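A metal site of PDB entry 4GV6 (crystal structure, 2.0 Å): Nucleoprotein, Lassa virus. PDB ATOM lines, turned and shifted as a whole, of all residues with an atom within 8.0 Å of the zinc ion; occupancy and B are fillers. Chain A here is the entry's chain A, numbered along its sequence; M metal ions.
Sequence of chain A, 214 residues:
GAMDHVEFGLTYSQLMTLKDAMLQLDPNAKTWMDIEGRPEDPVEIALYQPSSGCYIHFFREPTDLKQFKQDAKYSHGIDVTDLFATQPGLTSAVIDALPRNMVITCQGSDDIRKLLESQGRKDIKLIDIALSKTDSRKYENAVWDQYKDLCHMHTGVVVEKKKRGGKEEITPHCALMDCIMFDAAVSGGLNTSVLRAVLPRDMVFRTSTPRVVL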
ATOM      1  N   GLU A  36       6.832   1.438  20.245  1.00  0.00           N
ATOM      2  CA  GLU A  36       5.746   1.918  21.092  1.00  0.00           C
ATOM      3  C   GLU A  36       6.263   3.129  21.860  1.00  0.00           C
ATOM      4  O   GLU A  36       7.437   3.194  22.201  1.00  0.00           O
ATOM      5  CB  GLU A  36       5.221   0.838  22.044  1.00  0.00           C
ATOM      6  CG  GLU A  36       4.795  -0.459  21.347  1.00  0.00           C
ATOM      7  CD  GLU A  36       3.758  -0.251  20.252  1.00  0.00           C
ATOM      8  OE1 GLU A  36       2.910   0.671  20.345  1.00  0.00           O
ATOM      9  OE2 GLU A  36       3.772  -1.044  19.276  1.00  0.00           O
ATOM     10  N   GLU A  44       9.412   1.266  23.674  1.00  0.00           N
ATOM     11  CA  GLU A  44       9.734  -0.055  23.146  1.00  0.00           C
ATOM     12  C   GLU A  44      10.168   0.074  21.691  1.00  0.00           C
ATOM     13  O   GLU A  44       9.541   0.801  20.896  1.00  0.00           O
ATOM     14  CB  GLU A  44       8.530  -0.997  23.260  1.00  0.00           C
ATOM     15  CG  GLU A  44       8.851  -2.441  22.885  1.00  0.00           C
ATOM     16  CD  GLU A  44       7.630  -3.324  22.838  1.00  0.00           C
ATOM     17  OE1 GLU A  44       6.545  -2.801  22.489  1.00  0.00           O
ATOM     18  OE2 GLU A  44       7.751  -4.545  23.132  1.00  0.00           O
ATOM     19  N   ILE A  45      11.263  -0.599  21.357  1.00  0.00           N
ATOM     20  CA  ILE A  45      11.788  -0.603  20.000  1.00  0.00           C
ATOM     21  C   ILE A  45      12.014  -2.037  19.521  1.00  0.00           C
ATOM     22  O   ILE A  45      12.515  -2.888  20.273  1.00  0.00           O
ATOM     23  CB  ILE A  45      13.086   0.240  19.918  1.00  0.00           C
ATOM     24  CG1 ILE A  45      12.752   1.715  20.189  1.00  0.00           C
ATOM     25  CG2 ILE A  45      13.743   0.082  18.548  1.00  0.00           C
ATOM     26  CD1 ILE A  45      13.953   2.595  20.378  1.00  0.00           C
ATOM     27  N   ALA A  46      11.625  -2.311  18.289  1.00  0.00           N
ATOM     28  CA  ALA A  46      11.863  -3.606  17.669  1.00  0.00           C
ATOM     29  C   ALA A  46      12.309  -3.448  16.224  1.00  0.00           C
ATOM     30  O   ALA A  46      11.792  -2.600  15.500  1.00  0.00           O
ATOM     31  CB  ALA A  46      10.618  -4.458  17.747  1.00  0.00           C
ATOM     32  N   HIS A  57      15.201  -6.169  20.065  1.00  0.00           N
ATOM     33  CA  HIS A  57      14.071  -5.816  20.916  1.00  0.00           C
ATOM     34  C   HIS A  57      14.568  -5.344  22.271  1.00  0.00           C
ATOM     35  O   HIS A  57      15.277  -6.065  22.964  1.00  0.00           O
ATOM     36  CB  HIS A  57      13.139  -7.029  21.075  1.00  0.00           C
ATOM     37  CG  HIS A  57      11.902  -6.758  21.872  1.00  0.00           C
ATOM     38  ND1 HIS A  57      11.414  -7.658  22.791  1.00  0.00           N
ATOM     39  CD2 HIS A  57      11.062  -5.694  21.906  1.00  0.00           C
ATOM     40  CE1 HIS A  57      10.313  -7.157  23.346  1.00  0.00           C
ATOM     41  NE2 HIS A  57      10.077  -5.970  22.822  1.00  0.00           N
ATOM     42  N   PHE A  58      14.190  -4.122  22.626  1.00  0.00           N
ATOM     43  CA  PHE A  58      14.573  -3.528  23.909  1.00  0.00           C
ATOM     44  C   PHE A  58      13.620  -2.415  24.313  1.00  0.00           C
ATOM     45  O   PHE A  58      12.782  -1.988  23.525  1.00  0.00           O
ATOM     46  CB  PHE A  58      16.011  -2.991  23.847  1.00  0.00           C
ATOM     47  CG  PHE A  58      16.225  -1.930  22.802  1.00  0.00           C
ATOM     48  CD1 PHE A  58      16.511  -2.272  21.491  1.00  0.00           C
ATOM     49  CD2 PHE A  58      16.153  -0.581  23.139  1.00  0.00           C
ATOM     50  CE1 PHE A  58      16.700  -1.298  20.534  1.00  0.00           C
ATOM     51  CE2 PHE A  58      16.355   0.392  22.187  1.00  0.00           C
ATOM     52  CZ  PHE A  58      16.628   0.036  20.873  1.00  0.00           C
ATOM     53  N   PHE A  59      13.768  -1.949  25.551  1.00  0.00           N
ATOM     54  CA  PHE A  59      12.848  -0.980  26.121  1.00  0.00           C
ATOM     55  C   PHE A  59      13.594   0.249  26.620  1.00  0.00           C
ATOM     56  O   PHE A  59      14.810   0.272  26.631  1.00  0.00           O
ATOM     57  CB  PHE A  59      12.069  -1.633  27.255  1.00  0.00           C
ATOM     58  CG  PHE A  59      11.356  -2.880  26.843  1.00  0.00           C
ATOM     59  CD1 PHE A  59      11.997  -4.115  26.887  1.00  0.00           C
ATOM     60  CD2 PHE A  59      10.047  -2.826  26.403  1.00  0.00           C
ATOM     61  CE1 PHE A  59      11.344  -5.268  26.491  1.00  0.00           C
ATOM     62  CE2 PHE A  59       9.374  -3.987  26.002  1.00  0.00           C
ATOM     63  CZ  PHE A  59      10.026  -5.207  26.058  1.00  0.00           C
ATOM     64  N   HIS A  76      -0.326   0.632  23.880  1.00  0.00           N
ATOM     65  CA  HIS A  76       0.680  -0.385  24.197  1.00  0.00           C
ATOM     66  C   HIS A  76       0.465  -1.137  25.496  1.00  0.00           C
ATOM     67  O   HIS A  76       0.968  -2.241  25.648  1.00  0.00           O
ATOM     68  CB  HIS A  76       2.105   0.180  24.127  1.00  0.00           C
ATOM     69  CG  HIS A  76       2.358   1.379  24.984  1.00  0.00           C
ATOM     70  ND1 HIS A  76       2.337   1.338  26.364  1.00  0.00           N
ATOM     71  CD2 HIS A  76       2.651   2.665  24.661  1.00  0.00           C
ATOM     72  CE1 HIS A  76       2.607   2.540  26.847  1.00  0.00           C
ATOM     73  NE2 HIS A  76       2.799   3.365  25.837  1.00  0.00           N
ATOM     74  N   ILE A  78       1.760  -1.010  28.396  1.00  0.00           N
ATOM     75  CA  ILE A  78       2.983  -1.401  29.086  1.00  0.00           C
ATOM     76  C   ILE A  78       2.947  -0.872  30.513  1.00  0.00           C
ATOM     77  O   ILE A  78       2.619   0.292  30.754  1.00  0.00           O
ATOM     78  CB  ILE A  78       4.249  -0.866  28.350  1.00  0.00           C
ATOM     79  CG1 ILE A  78       4.327  -1.452  26.933  1.00  0.00           C
ATOM     80  CG2 ILE A  78       5.519  -1.233  29.125  1.00  0.00           C
ATOM     81  CD1 ILE A  78       5.393  -0.838  26.051  1.00  0.00           C
ATOM     82  N   TRP A 144       0.567 -13.599  18.045  1.00  0.00           N
ATOM     83  CA  TRP A 144       0.549 -13.671  19.515  1.00  0.00           C
ATOM     84  C   TRP A 144       0.488 -15.126  20.005  1.00  0.00           C
ATOM     85  O   TRP A 144       1.185 -15.486  20.963  1.00  0.00           O
ATOM     86  CB  TRP A 144      -0.613 -12.878  20.108  1.00  0.00           C
ATOM     87  CG  TRP A 144      -0.368 -11.365  20.225  1.00  0.00           C
ATOM     88  CD1 TRP A 144      -0.874 -10.390  19.435  1.00  0.00           C
ATOM     89  CD2 TRP A 144       0.414 -10.693  21.241  1.00  0.00           C
ATOM     90  NE1 TRP A 144      -0.451  -9.157  19.855  1.00  0.00           N
ATOM     91  CE2 TRP A 144       0.335  -9.306  20.970  1.00  0.00           C
ATOM     92  CE3 TRP A 144       1.171 -11.121  22.342  1.00  0.00           C
ATOM     93  CZ2 TRP A 144       0.985  -8.354  21.750  1.00  0.00           C
ATOM     94  CZ3 TRP A 144       1.817 -10.177  23.111  1.00  0.00           C
ATOM     95  CH2 TRP A 144       1.717  -8.808  22.815  1.00  0.00           C
ATOM     96  N   LYS A 148       4.005 -15.084  21.901  1.00  0.00           N
ATOM     97  CA  LYS A 148       3.709 -14.400  23.154  1.00  0.00           C
ATOM     98  C   LYS A 148       4.863 -14.399  24.172  1.00  0.00           C
ATOM     99  O   LYS A 148       5.099 -13.392  24.849  1.00  0.00           O
ATOM    100  CB  LYS A 148       2.432 -14.952  23.805  1.00  0.00           C
ATOM    101  CG  LYS A 148       2.388 -16.461  23.928  1.00  0.00           C
ATOM    102  CD  LYS A 148       1.111 -16.918  24.598  1.00  0.00           C
ATOM    103  CE  LYS A 148       1.086 -18.427  24.780  1.00  0.00           C
ATOM    104  NZ  LYS A 148       0.521 -19.130  23.613  1.00  0.00           N
ATOM    105  N   LEU A 150       7.902 -14.036  23.812  1.00  0.00           N
ATOM    106  CA  LEU A 150       8.982 -13.120  23.474  1.00  0.00           C
ATOM    107  C   LEU A 150       8.798 -11.698  24.031  1.00  0.00           C
ATOM    108  O   LEU A 150       9.757 -10.916  24.021  1.00  0.00           O
ATOM    109  CB  LEU A 150       9.171 -13.051  21.952  1.00  0.00           C
ATOM    110  CG  LEU A 150       9.494 -14.354  21.222  1.00  0.00           C
ATOM    111  CD1 LEU A 150       9.733 -14.046  19.746  1.00  0.00           C
ATOM    112  CD2 LEU A 150      10.701 -15.054  21.832  1.00  0.00           C
ATOM    113  N   CYS A 151       7.601 -11.370  24.495  1.00  0.00           N
ATOM    114  CA  CYS A 151       7.359 -10.100  25.202  1.00  0.00           C
ATOM    115  C   CYS A 151       6.255 -10.213  26.259  1.00  0.00           C
ATOM    116  O   CYS A 151       5.130 -10.597  25.944  1.00  0.00           O
ATOM    117  CB  CYS A 151       6.976  -9.002  24.222  1.00  0.00           C
ATOM    118  SG  CYS A 151       7.145  -7.357  24.920  1.00  0.00           S
ATOM    119  N   HIS A 152       6.590  -9.845  27.494  1.00  0.00           N
ATOM    120  CA  HIS A 152       5.660  -9.944  28.635  1.00  0.00           C
ATOM    121  C   HIS A 152       5.231  -8.581  29.198  1.00  0.00           C
ATOM    122  O   HIS A 152       4.592  -8.513  30.247  1.00  0.00           O
ATOM    123  CB  HIS A 152       6.288 -10.772  29.770  1.00  0.00           C
ATOM    124  CG  HIS A 152       6.772 -12.123  29.317  1.00  0.00           C
ATOM    125  ND1 HIS A 152       6.036 -13.265  29.506  1.00  0.00           N
ATOM    126  CD2 HIS A 152       7.910 -12.492  28.682  1.00  0.00           C
ATOM    127  CE1 HIS A 152       6.698 -14.291  29.012  1.00  0.00           C
ATOM    128  NE2 HIS A 152       7.837 -13.853  28.502  1.00  0.00           N
ATOM    129  N   MET A 153       5.555  -7.510  28.470  1.00  0.00           N
ATOM    130  CA  MET A 153       5.381  -6.146  28.974  1.00  0.00           C
ATOM    131  C   MET A 153       3.977  -5.578  28.869  1.00  0.00           C
ATOM    132  O   MET A 153       3.666  -4.583  29.527  1.00  0.00           O
ATOM    133  CB  MET A 153       6.342  -5.204  28.248  1.00  0.00           C
ATOM    134  CG  MET A 153       7.798  -5.408  28.648  1.00  0.00           C
ATOM    135  SD  MET A 153       8.248  -4.585  30.185  1.00  0.00           S
ATOM    136  CE  MET A 153       9.988  -5.009  30.248  1.00  0.00           C
ATOM    137  N   HIS A 154       3.116  -6.194  28.064  1.00  0.00           N
ATOM    138  CA  HIS A 154       1.830  -5.601  27.718  1.00  0.00           C
ATOM    139  C   HIS A 154       0.695  -6.207  28.536  1.00  0.00           C
ATOM    140  O   HIS A 154      -0.109  -6.986  28.034  1.00  0.00           O
ATOM    141  CB  HIS A 154       1.603  -5.735  26.211  1.00  0.00           C
ATOM    142  CG  HIS A 154       2.775  -5.265  25.401  1.00  0.00           C
ATOM    143  ND1 HIS A 154       2.883  -3.976  24.958  1.00  0.00           N
ATOM    144  CD2 HIS A 154       3.902  -5.903  25.009  1.00  0.00           C
ATOM    145  CE1 HIS A 154       4.021  -3.835  24.297  1.00  0.00           C
ATOM    146  NE2 HIS A 154       4.649  -4.996  24.306  1.00  0.00           N
ATOM    147  N   PRO A 172      -3.272  -5.439  23.126  1.00  0.00           N
ATOM    148  CA  PRO A 172      -2.223  -4.416  23.176  1.00  0.00           C
ATOM    149  C   PRO A 172      -1.272  -4.439  21.973  1.00  0.00           C
ATOM    150  O   PRO A 172      -1.049  -5.482  21.368  1.00  0.00           O
ATOM    151  CB  PRO A 172      -1.460  -4.780  24.449  1.00  0.00           C
ATOM    152  CG  PRO A 172      -2.461  -5.454  25.317  1.00  0.00           C
ATOM    153  CD  PRO A 172      -3.352  -6.215  24.374  1.00  0.00           C
ATOM    154  N   HIS A 173      -0.722  -3.275  21.640  1.00  0.00           N
ATOM    155  CA  HIS A 173       0.262  -3.140  20.564  1.00  0.00           C
ATOM    156  C   HIS A 173       1.660  -3.340  21.103  1.00  0.00           C
ATOM    157  O   HIS A 173       2.104  -2.612  21.987  1.00  0.00           O
ATOM    158  CB  HIS A 173       0.140  -1.763  19.922  1.00  0.00           C
ATOM    159  CG  HIS A 173      -1.122  -1.570  19.130  1.00  0.00           C
ATOM    160  ND1 HIS A 173      -1.295  -0.513  18.262  1.00  0.00           N
ATOM    161  CD2 HIS A 173      -2.254  -2.309  19.049  1.00  0.00           C
ATOM    162  CE1 HIS A 173      -2.488  -0.592  17.696  1.00  0.00           C
ATOM    163  NE2 HIS A 173      -3.084  -1.676  18.152  1.00  0.00           N
ATOM    164  N   CYS A 174       2.364  -4.343  20.566  1.00  0.00           N
ATOM    165  CA  CYS A 174       3.743  -4.656  20.883  1.00  0.00           C
ATOM    166  C   CYS A 174       4.594  -4.394  19.655  1.00  0.00           C
ATOM    167  O   CYS A 174       4.249  -4.859  18.556  1.00  0.00           O
ATOM    168  CB  CYS A 174       3.903  -6.118  21.305  1.00  0.00           C
ATOM    169  SG  CYS A 174       5.609  -6.698  21.484  1.00  0.00           S
ATOM    170  N   ALA A 175       5.690  -3.649  19.829  1.00  0.00           N
ATOM    171  CA  ALA A 175       6.585  -3.324  18.722  1.00  0.00           C
ATOM    172  C   ALA A 175       7.081  -4.573  18.006  1.00  0.00           C
ATOM    173  O   ALA A 175       7.238  -4.551  16.786  1.00  0.00           O
ATOM    174  CB  ALA A 175       7.753  -2.472  19.189  1.00  0.00           C
ATOM    175  N   LEU A 176       7.342  -5.640  18.754  1.00  0.00           N
ATOM    176  CA  LEU A 176       7.865  -6.870  18.192  1.00  0.00           C
ATOM    177  C   LEU A 176       6.775  -7.674  17.490  1.00  0.00           C
ATOM    178  O   LEU A 176       6.933  -8.058  16.334  1.00  0.00           O
ATOM    179  CB  LEU A 176       8.583  -7.702  19.250  1.00  0.00           C
ATOM    180  CG  LEU A 176       9.203  -9.011  18.759  1.00  0.00           C
ATOM    181  CD1 LEU A 176      10.169  -8.801  17.594  1.00  0.00           C
ATOM    182  CD2 LEU A 176       9.881  -9.737  19.918  1.00  0.00           C
ATOM    183  N   MET A 177       5.655  -7.919  18.170  1.00  0.00           N
ATOM    184  CA  MET A 177       4.538  -8.627  17.551  1.00  0.00           C
ATOM    185  C   MET A 177       4.047  -7.887  16.312  1.00  0.00           C
ATOM    186  O   MET A 177       3.678  -8.516  15.322  1.00  0.00           O
ATOM    187  CB  MET A 177       3.384  -8.862  18.536  1.00  0.00           C
ATOM    188  CG  MET A 177       3.778  -9.544  19.823  1.00  0.00           C
ATOM    189  SD  MET A 177       4.633 -11.110  19.596  1.00  0.00           S
ATOM    190  CE  MET A 177       5.739 -11.097  20.988  1.00  0.00           C
ATOM    191  N   ASP A 178       4.040  -6.554  16.365  1.00  0.00           N
ATOM    192  CA  ASP A 178       3.665  -5.729  15.203  1.00  0.00           C
ATOM    193  C   ASP A 178       4.547  -6.018  13.972  1.00  0.00           C
ATOM    194  O   ASP A 178       4.021  -6.283  12.897  1.00  0.00           O
ATOM    195  CB  ASP A 178       3.704  -4.234  15.533  1.00  0.00           C
ATOM    196  CG  ASP A 178       2.417  -3.723  16.189  1.00  0.00           C
ATOM    197  OD1 ASP A 178       1.508  -4.530  16.470  1.00  0.00           O
ATOM    198  OD2 ASP A 178       2.321  -2.502  16.419  1.00  0.00           O
HETATM  199 ZN    ZN M   1       6.267  -5.909  23.458  1.00  0.00          ZN
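The side-chain sulfur (SG) of Cys 174 sits close to the backbone NH (N) of Met 177 (3.5 Å). A ring nitrogen (ND1) of His 154 sits at hydrogen-bond distance from the backbone carbonyl oxygen (O) of His 76, at 2.7 Å. OE1 of Glu 44 sits at hydrogen-bond distance from N of Ala 175 (2.9 Å). OE2 of Glu 44 lies close to NE2 of His 57. The backbone carbonyl oxygen (O) of Glu 44 lies within hydrogen-bond range of the backbone NH (N) of Glu 36 (2.9 Å). ND1 of His 154 lies close to O of His 173 (3.4 Å). N of Leu 176 lies close to SG of Cys 174, at 3.4 Å.
NE2 of His 57 touches the zinc ion, 3.9 Å away. Five residues have an atom within 4 Å of the zinc ion: Glu 44, His 57, Cys 151, His 154 and Cys 174. The nearest printed residue that does not touch the zinc ion is Ala 175 (4.3 Å).
The zinc ion is bound by OE2 of Glu 44, at 2.0 Å. The zinc ion is bound by NE2 of His 154. SG of Cys 174 binds the zinc ion, 2.2 Å away. The zinc ion is bound by the side-chain sulfur (SG) of Cys 151 (2.2 Å). The zinc ion has four donor atoms within binding distance.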
